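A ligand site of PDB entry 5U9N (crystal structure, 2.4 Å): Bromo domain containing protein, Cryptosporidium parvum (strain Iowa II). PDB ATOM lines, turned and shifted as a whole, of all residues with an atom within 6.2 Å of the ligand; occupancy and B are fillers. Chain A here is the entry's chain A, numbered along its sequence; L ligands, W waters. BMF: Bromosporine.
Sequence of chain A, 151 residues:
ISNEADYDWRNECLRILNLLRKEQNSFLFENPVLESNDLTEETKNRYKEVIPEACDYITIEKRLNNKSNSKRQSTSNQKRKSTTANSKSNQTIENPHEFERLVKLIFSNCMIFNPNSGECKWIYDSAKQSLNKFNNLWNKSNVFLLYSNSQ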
ATOM      1  N   PHE A  27      28.134  -7.100   8.830  1.00  0.00           N
ATOM      2  CA  PHE A  27      29.303  -6.305   8.411  1.00  0.00           C
ATOM      3  C   PHE A  27      29.072  -5.666   7.021  1.00  0.00           C
ATOM      4  O   PHE A  27      29.642  -4.612   6.739  1.00  0.00           O
ATOM      5  CB  PHE A  27      30.586  -7.175   8.393  1.00  0.00           C
ATOM      6  CG  PHE A  27      30.634  -8.229   7.302  1.00  0.00           C
ATOM      7  CD1 PHE A  27      31.154  -7.935   6.062  1.00  0.00           C
ATOM      8  CD2 PHE A  27      30.165  -9.511   7.537  1.00  0.00           C
ATOM      9  CE1 PHE A  27      31.176  -8.902   5.051  1.00  0.00           C
ATOM     10  CE2 PHE A  27      30.151 -10.456   6.515  1.00  0.00           C
ATOM     11  CZ  PHE A  27      30.657 -10.145   5.281  1.00  0.00           C
ATOM     12  N   LEU A  28      28.238  -6.295   6.168  1.00  0.00           N
ATOM     13  CA  LEU A  28      27.964  -5.785   4.815  1.00  0.00           C
ATOM     14  C   LEU A  28      27.407  -4.362   4.843  1.00  0.00           C
ATOM     15  O   LEU A  28      27.787  -3.540   4.023  1.00  0.00           O
ATOM     16  CB  LEU A  28      26.957  -6.691   4.074  1.00  0.00           C
ATOM     17  CG  LEU A  28      27.437  -8.113   3.701  1.00  0.00           C
ATOM     18  CD1 LEU A  28      26.276  -8.948   3.144  1.00  0.00           C
ATOM     19  CD2 LEU A  28      28.558  -8.061   2.688  1.00  0.00           C
ATOM     20  N   PHE A  29      26.536  -4.081   5.816  1.00  0.00           N
ATOM     21  CA  PHE A  29      25.816  -2.831   5.883  1.00  0.00           C
ATOM     22  C   PHE A  29      26.340  -1.865   6.936  1.00  0.00           C
ATOM     23  O   PHE A  29      25.684  -0.846   7.198  1.00  0.00           O
ATOM     24  CB  PHE A  29      24.364  -3.154   6.207  1.00  0.00           C
ATOM     25  CG  PHE A  29      23.845  -4.384   5.492  1.00  0.00           C
ATOM     26  CD1 PHE A  29      23.602  -4.364   4.132  1.00  0.00           C
ATOM     27  CD2 PHE A  29      23.681  -5.579   6.183  1.00  0.00           C
ATOM     28  CE1 PHE A  29      23.131  -5.495   3.475  1.00  0.00           C
ATOM     29  CE2 PHE A  29      23.197  -6.714   5.525  1.00  0.00           C
ATOM     30  CZ  PHE A  29      22.915  -6.654   4.179  1.00  0.00           C
ATOM     31  N   GLU A  30      27.511  -2.141   7.524  1.00  0.00           N
ATOM     32  CA  GLU A  30      28.023  -1.334   8.630  1.00  0.00           C
ATOM     33  C   GLU A  30      28.624  -0.015   8.147  1.00  0.00           C
ATOM     34  O   GLU A  30      28.236   1.037   8.645  1.00  0.00           O
ATOM     35  CB  GLU A  30      29.071  -2.127   9.423  1.00  0.00           C
ATOM     36  CG  GLU A  30      29.585  -1.436  10.664  1.00  0.00           C
ATOM     37  CD  GLU A  30      28.512  -0.911  11.603  1.00  0.00           C
ATOM     38  OE1 GLU A  30      27.466  -1.588  11.732  1.00  0.00           O
ATOM     39  OE2 GLU A  30      28.717   0.159  12.207  1.00  0.00           O
ATOM     40  N   ASN A  31      29.539  -0.068   7.204  1.00  0.00           N
ATOM     41  CA  ASN A  31      30.235   1.123   6.734  1.00  0.00           C
ATOM     42  C   ASN A  31      29.926   1.388   5.268  1.00  0.00           C
ATOM     43  O   ASN A  31      29.473   0.478   4.574  1.00  0.00           O
ATOM     44  CB  ASN A  31      31.751   0.969   6.939  1.00  0.00           C
ATOM     45  CG  ASN A  31      32.097   0.628   8.379  1.00  0.00           C
ATOM     46  OD1 ASN A  31      31.750   1.366   9.316  1.00  0.00           O
ATOM     47  ND2 ASN A  31      32.721  -0.530   8.581  1.00  0.00           N
ATOM     48  N   PRO A  32      30.171   2.627   4.770  1.00  0.00           N
ATOM     49  CA  PRO A  32      29.863   2.912   3.360  1.00  0.00           C
ATOM     50  C   PRO A  32      30.607   2.032   2.370  1.00  0.00           C
ATOM     51  O   PRO A  32      31.831   1.888   2.467  1.00  0.00           O
ATOM     52  CB  PRO A  32      30.269   4.391   3.195  1.00  0.00           C
ATOM     53  CG  PRO A  32      30.240   4.948   4.569  1.00  0.00           C
ATOM     54  CD  PRO A  32      30.673   3.826   5.462  1.00  0.00           C
ATOM     55  N   VAL A  33      29.873   1.461   1.398  1.00  0.00           N
ATOM     56  CA  VAL A  33      30.452   0.620   0.348  1.00  0.00           C
ATOM     57  C   VAL A  33      31.415   1.422  -0.548  1.00  0.00           C
ATOM     58  O   VAL A  33      32.413   0.874  -1.010  1.00  0.00           O
ATOM     59  CB  VAL A  33      29.375  -0.101  -0.531  1.00  0.00           C
ATOM     60  CG1 VAL A  33      28.603  -1.133   0.271  1.00  0.00           C
ATOM     61  CG2 VAL A  33      28.414   0.888  -1.179  1.00  0.00           C
ATOM     62  N   LEU A  34      31.100   2.709  -0.806  1.00  0.00           N
ATOM     63  CA  LEU A  34      31.932   3.563  -1.652  1.00  0.00           C
ATOM     64  C   LEU A  34      33.267   3.983  -0.959  1.00  0.00           C
ATOM     65  O   LEU A  34      34.187   4.385  -1.657  1.00  0.00           O
ATOM     66  CB  LEU A  34      31.154   4.813  -2.086  1.00  0.00           C
ATOM     67  CG  LEU A  34      29.907   4.573  -2.969  1.00  0.00           C
ATOM     68  CD1 LEU A  34      29.164   5.866  -3.201  1.00  0.00           C
ATOM     69  CD2 LEU A  34      30.299   3.941  -4.314  1.00  0.00           C
ATOM     70  N   SER A  36      34.814   1.638   0.993  1.00  0.00           N
ATOM     71  CA  SER A  36      35.413   0.346   1.291  1.00  0.00           C
ATOM     72  C   SER A  36      36.640   0.044   0.424  1.00  0.00           C
ATOM     73  O   SER A  36      36.560   0.044  -0.804  1.00  0.00           O
ATOM     74  CB  SER A  36      34.380  -0.772   1.108  1.00  0.00           C
ATOM     75  OG  SER A  36      34.870  -2.006   1.627  1.00  0.00           O
ATOM     76  N   ASN A  37      37.767  -0.307   1.087  1.00  0.00           N
ATOM     77  CA  ASN A  37      38.994  -0.718   0.410  1.00  0.00           C
ATOM     78  C   ASN A  37      38.898  -2.219   0.034  1.00  0.00           C
ATOM     79  O   ASN A  37      39.714  -2.717  -0.739  1.00  0.00           O
ATOM     80  CB  ASN A  37      40.217  -0.486   1.319  1.00  0.00           C
ATOM     81  CG  ASN A  37      40.364   0.940   1.799  1.00  0.00           C
ATOM     82  OD1 ASN A  37      39.836   1.880   1.200  1.00  0.00           O
ATOM     83  ND2 ASN A  37      41.090   1.122   2.897  1.00  0.00           N
ATOM     84  N   ASP A  38      37.902  -2.947   0.622  1.00  0.00           N
ATOM     85  CA  ASP A  38      37.690  -4.372   0.354  1.00  0.00           C
ATOM     86  C   ASP A  38      37.199  -4.587  -1.082  1.00  0.00           C
ATOM     87  O   ASP A  38      37.741  -5.447  -1.781  1.00  0.00           O
ATOM     88  CB  ASP A  38      36.688  -4.976   1.374  1.00  0.00           C
ATOM     89  CG  ASP A  38      37.165  -4.898   2.824  1.00  0.00           C
ATOM     90  OD1 ASP A  38      37.884  -5.834   3.268  1.00  0.00           O
ATOM     91  OD2 ASP A  38      36.802  -3.924   3.523  1.00  0.00           O
ATOM     92  N   LEU A  39      36.256  -3.763  -1.535  1.00  0.00           N
ATOM     93  CA  LEU A  39      35.739  -3.859  -2.910  1.00  0.00           C
ATOM     94  C   LEU A  39      36.733  -3.244  -3.899  1.00  0.00           C
ATOM     95  O   LEU A  39      37.583  -2.431  -3.504  1.00  0.00           O
ATOM     96  CB  LEU A  39      34.378  -3.152  -3.020  1.00  0.00           C
ATOM     97  CG  LEU A  39      33.185  -3.845  -2.337  1.00  0.00           C
ATOM     98  CD1 LEU A  39      32.943  -3.289  -0.945  1.00  0.00           C
ATOM     99  CD2 LEU A  39      31.922  -3.711  -3.175  1.00  0.00           C
ATOM    100  N   THR A  43      33.824  -2.355  -9.370  1.00  0.00           N
ATOM    101  CA  THR A  43      32.533  -2.623  -8.735  1.00  0.00           C
ATOM    102  C   THR A  43      31.953  -1.346  -8.062  1.00  0.00           C
ATOM    103  O   THR A  43      30.746  -1.140  -8.108  1.00  0.00           O
ATOM    104  CB  THR A  43      32.688  -3.775  -7.703  1.00  0.00           C
ATOM    105  OG1 THR A  43      33.771  -3.477  -6.824  1.00  0.00           O
ATOM    106  CG2 THR A  43      32.951  -5.121  -8.368  1.00  0.00           C
ATOM    107  N   ARG A  46      30.447   0.988 -10.791  1.00  0.00           N
ATOM    108  CA  ARG A  46      29.146   0.521 -11.266  1.00  0.00           C
ATOM    109  C   ARG A  46      28.102   0.832 -10.197  1.00  0.00           C
ATOM    110  O   ARG A  46      26.979   1.184 -10.537  1.00  0.00           O
ATOM    111  CB  ARG A  46      29.178  -0.996 -11.592  1.00  0.00           C
ATOM    112  CG  ARG A  46      27.841  -1.511 -12.188  1.00  0.00           C
ATOM    113  CD  ARG A  46      27.867  -2.988 -12.574  1.00  0.00           C
ATOM    114  NE  ARG A  46      27.951  -3.880 -11.406  1.00  0.00           N
ATOM    115  CZ  ARG A  46      29.076  -4.403 -10.902  1.00  0.00           C
ATOM    116  NH1 ARG A  46      29.032  -5.210  -9.855  1.00  0.00           N
ATOM    117  NH2 ARG A  46      30.253  -4.119 -11.457  1.00  0.00           N
ATOM    118  N   TYR A  47      28.485   0.783  -8.906  1.00  0.00           N
ATOM    119  CA  TYR A  47      27.587   1.068  -7.783  1.00  0.00           C
ATOM    120  C   TYR A  47      27.031   2.496  -7.836  1.00  0.00           C
ATOM    121  O   TYR A  47      25.858   2.682  -7.554  1.00  0.00           O
ATOM    122  CB  TYR A  47      28.313   0.863  -6.434  1.00  0.00           C
ATOM    123  CG  TYR A  47      27.360   0.772  -5.269  1.00  0.00           C
ATOM    124  CD1 TYR A  47      26.799  -0.429  -4.889  1.00  0.00           C
ATOM    125  CD2 TYR A  47      27.041   1.904  -4.515  1.00  0.00           C
ATOM    126  CE1 TYR A  47      25.939  -0.516  -3.804  1.00  0.00           C
ATOM    127  CE2 TYR A  47      26.152   1.840  -3.452  1.00  0.00           C
ATOM    128  CZ  TYR A  47      25.589   0.616  -3.111  1.00  0.00           C
ATOM    129  OH  TYR A  47      24.742   0.513  -2.032  1.00  0.00           O
ATOM    130  N   ILE A 106      19.053   0.842   2.847  1.00  0.00           N
ATOM    131  CA  ILE A 106      20.247  -0.006   2.931  1.00  0.00           C
ATOM    132  C   ILE A 106      19.952  -1.370   2.314  1.00  0.00           C
ATOM    133  O   ILE A 106      20.766  -1.893   1.566  1.00  0.00           O
ATOM    134  CB  ILE A 106      20.681  -0.170   4.443  1.00  0.00           C
ATOM    135  CG1 ILE A 106      21.212   1.147   4.996  1.00  0.00           C
ATOM    136  CG2 ILE A 106      21.752  -1.279   4.615  1.00  0.00           C
ATOM    137  CD1 ILE A 106      21.458   1.134   6.503  1.00  0.00           C
ATOM    138  N   ASN A 109      18.895  -1.112  -1.648  1.00  0.00           N
ATOM    139  CA  ASN A 109      20.053  -0.836  -2.509  1.00  0.00           C
ATOM    140  C   ASN A 109      20.852  -2.128  -2.723  1.00  0.00           C
ATOM    141  O   ASN A 109      21.249  -2.448  -3.842  1.00  0.00           O
ATOM    142  CB  ASN A 109      20.966   0.229  -1.887  1.00  0.00           C
ATOM    143  CG  ASN A 109      20.388   1.618  -1.894  1.00  0.00           C
ATOM    144  OD1 ASN A 109      19.384   1.897  -2.557  1.00  0.00           O
ATOM    145  ND2 ASN A 109      21.011   2.519  -1.153  1.00  0.00           N
ATOM    146  N   CYS A 110      21.019  -2.895  -1.660  1.00  0.00           N
ATOM    147  CA  CYS A 110      21.715  -4.163  -1.720  1.00  0.00           C
ATOM    148  C   CYS A 110      20.951  -5.159  -2.584  1.00  0.00           C
ATOM    149  O   CYS A 110      21.566  -5.908  -3.332  1.00  0.00           O
ATOM    150  CB  CYS A 110      21.939  -4.702  -0.317  1.00  0.00           C
ATOM    151  SG  CYS A 110      22.797  -6.277  -0.267  1.00  0.00           S
ATOM    152  N   PHE A 113      21.359  -3.961  -6.361  1.00  0.00           N
ATOM    153  CA  PHE A 113      22.704  -4.094  -6.902  1.00  0.00           C
ATOM    154  C   PHE A 113      23.173  -5.552  -7.030  1.00  0.00           C
ATOM    155  O   PHE A 113      23.958  -5.849  -7.935  1.00  0.00           O
ATOM    156  CB  PHE A 113      23.708  -3.319  -6.010  1.00  0.00           C
ATOM    157  CG  PHE A 113      25.101  -3.186  -6.592  1.00  0.00           C
ATOM    158  CD1 PHE A 113      25.331  -2.375  -7.689  1.00  0.00           C
ATOM    159  CD2 PHE A 113      26.177  -3.868  -6.038  1.00  0.00           C
ATOM    160  CE1 PHE A 113      26.613  -2.274  -8.261  1.00  0.00           C
ATOM    161  CE2 PHE A 113      27.443  -3.785  -6.614  1.00  0.00           C
ATOM    162  CZ  PHE A 113      27.666  -2.972  -7.717  1.00  0.00           C
ATOM    163  N   ASN A 114      22.755  -6.445  -6.123  1.00  0.00           N
ATOM    164  CA  ASN A 114      23.283  -7.816  -6.128  1.00  0.00           C
ATOM    165  C   ASN A 114      22.239  -8.790  -6.619  1.00  0.00           C
ATOM    166  O   ASN A 114      21.047  -8.556  -6.444  1.00  0.00           O
ATOM    167  CB  ASN A 114      23.786  -8.222  -4.726  1.00  0.00           C
ATOM    168  CG  ASN A 114      24.781  -7.223  -4.148  1.00  0.00           C
ATOM    169  OD1 ASN A 114      25.964  -7.264  -4.437  1.00  0.00           O
ATOM    170  ND2 ASN A 114      24.314  -6.278  -3.379  1.00  0.00           N
ATOM    171  N   PRO A 115      22.680  -9.881  -7.311  1.00  0.00           N
ATOM    172  CA  PRO A 115      21.702 -10.827  -7.875  1.00  0.00           C
ATOM    173  C   PRO A 115      21.156 -11.790  -6.836  1.00  0.00           C
ATOM    174  O   PRO A 115      21.834 -12.078  -5.836  1.00  0.00           O
ATOM    175  CB  PRO A 115      22.516 -11.554  -8.944  1.00  0.00           C
ATOM    176  CG  PRO A 115      23.896 -11.601  -8.383  1.00  0.00           C
ATOM    177  CD  PRO A 115      24.066 -10.294  -7.632  1.00  0.00           C
ATOM    178  N   CYS A 120      27.167 -15.799  -5.529  1.00  0.00           N
ATOM    179  CA  CYS A 120      27.205 -14.737  -4.541  1.00  0.00           C
ATOM    180  C   CYS A 120      25.765 -14.177  -4.263  1.00  0.00           C
ATOM    181  O   CYS A 120      25.606 -13.021  -3.897  1.00  0.00           O
ATOM    182  CB  CYS A 120      28.183 -13.632  -4.967  1.00  0.00           C
ATOM    183  SG  CYS A 120      29.923 -13.910  -4.399  1.00  0.00           S
ATOM    184  N   ILE A 123      24.637 -12.359  -0.563  1.00  0.00           N
ATOM    185  CA  ILE A 123      24.644 -10.927  -0.251  1.00  0.00           C
ATOM    186  C   ILE A 123      23.217 -10.425  -0.272  1.00  0.00           C
ATOM    187  O   ILE A 123      22.757  -9.878   0.716  1.00  0.00           O
ATOM    188  CB  ILE A 123      25.553 -10.129  -1.245  1.00  0.00           C
ATOM    189  CG1 ILE A 123      27.014 -10.533  -1.050  1.00  0.00           C
ATOM    190  CG2 ILE A 123      25.386  -8.635  -1.037  1.00  0.00           C
ATOM    191  CD1 ILE A 123      27.912  -9.969  -2.019  1.00  0.00           C
HETATM  192  C10 BMF L   1      30.758  -5.687   1.055  1.00  0.00           C
HETATM  193  N12 BMF L   1      28.620  -4.849   0.518  1.00  0.00           N
HETATM  194  C15 BMF L   1      28.626  -6.053  -2.100  1.00  0.00           C
HETATM  195  C17 BMF L   1      29.549  -7.174  -4.139  1.00  0.00           C
HETATM  196  C20 BMF L   1      30.029  -9.647  -6.133  1.00  0.00           C
HETATM  197  C22 BMF L   1      29.659  -6.177  -1.202  1.00  0.00           C
HETATM  198  C26 BMF L   1      26.090  -3.322   1.053  1.00  0.00           C
HETATM  199  C28 BMF L   1      32.850  -6.663   1.744  1.00  0.00           C
HETATM  200  C01 BMF L   1      33.969  -6.078   3.929  1.00  0.00           C
HETATM  201  C02 BMF L   1      32.850  -5.931   2.935  1.00  0.00           C
HETATM  202  C03 BMF L   1      31.762  -5.070   3.165  1.00  0.00           C
HETATM  203  N04 BMF L   1      31.678  -4.318   4.369  1.00  0.00           N
HETATM  204  S05 BMF L   1      32.014  -2.729   4.512  1.00  0.00           S
HETATM  205  C06 BMF L   1      31.163  -1.908   3.223  1.00  0.00           C
HETATM  206  O07 BMF L   1      31.451  -2.305   5.762  1.00  0.00           O
HETATM  207  O08 BMF L   1      33.412  -2.574   4.307  1.00  0.00           O
HETATM  208  C09 BMF L   1      30.724  -4.962   2.236  1.00  0.00           C
HETATM  209  C11 BMF L   1      29.641  -5.560   0.099  1.00  0.00           C
HETATM  210  N13 BMF L   1      27.590  -4.731  -0.386  1.00  0.00           N
HETATM  211  C14 BMF L   1      27.520  -5.257  -1.658  1.00  0.00           C
HETATM  212  N16 BMF L   1      28.535  -6.590  -3.416  1.00  0.00           N
HETATM  213  O18 BMF L   1      29.076  -7.565  -5.352  1.00  0.00           O
HETATM  214  C19 BMF L   1      30.040  -8.143  -6.290  1.00  0.00           C
HETATM  215  O21 BMF L   1      30.686  -7.347  -3.749  1.00  0.00           O
HETATM  216  N23 BMF L   1      26.387  -4.839  -2.224  1.00  0.00           N
HETATM  217  N24 BMF L   1      25.727  -4.043  -1.303  1.00  0.00           N
HETATM  218  C25 BMF L   1      26.444  -4.003  -0.214  1.00  0.00           C
HETATM  219  C27 BMF L   1      31.827  -6.537   0.819  1.00  0.00           C
HETATM  220  O   HOH W   1      24.010  -1.982  -1.350  1.00  0.00           O
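ND2 of Asn 114 lies within hydrogen-bond range of N23 of the ligand (2.8 Å).
N04 of the ligand is in hydrogen-bond range of O of Phe 27 (3.1 Å).
The side-chain hydroxyl of Ser 36 lies within hydrogen-bond range of an oxygen (O08) of the ligand (3.1 Å).
O07 of the ligand lies within hydrogen-bond range of N of Asn 31.
The side-chain amide nitrogen (ND2) of Asn 114 lies within hydrogen-bond range of the backbone carbonyl oxygen (O) of Cys 110, at 2.8 Å.
The side-chain carboxylate (OD2) of Asp 38 is in hydrogen-bond range of the side-chain hydroxyl (OG) of Ser 36.
SG of Cys 110 sits close to O of Ile 123 (3.7 Å).
Merely in contact with the ligand: Val 33 (3.4 Å), Leu 28 (3.4 Å), Asp 38 (3.6 Å), Ile 123 (3.7 Å), Leu 39 (3.8 Å), Cys 110 (3.8 Å), Pro 32 (3.9 Å) and Phe 113 (3.9 Å).
Hydrophobic or aromatic side chains that line the ligand: Phe 27, Leu 28, Val 33, Leu 39, Phe 113 and Ile 123.
12 residues have an atom within 4 Å of the ligand: Phe 27, Leu 28, Asn 31, Pro 32, Val 33, Ser 36, Asp 38, Leu 39, Cys 110, Phe 113, Asn 114 and Ile 123.
The nearest printed residue that does not touch the ligand is Phe 29 (4.1 Å).
Water W1 lies within hydrogen-bond range of N24 of the ligand (2.7 Å), OH of Tyr 47 (2.7 Å) and N of Cys 110 (3.1 Å).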
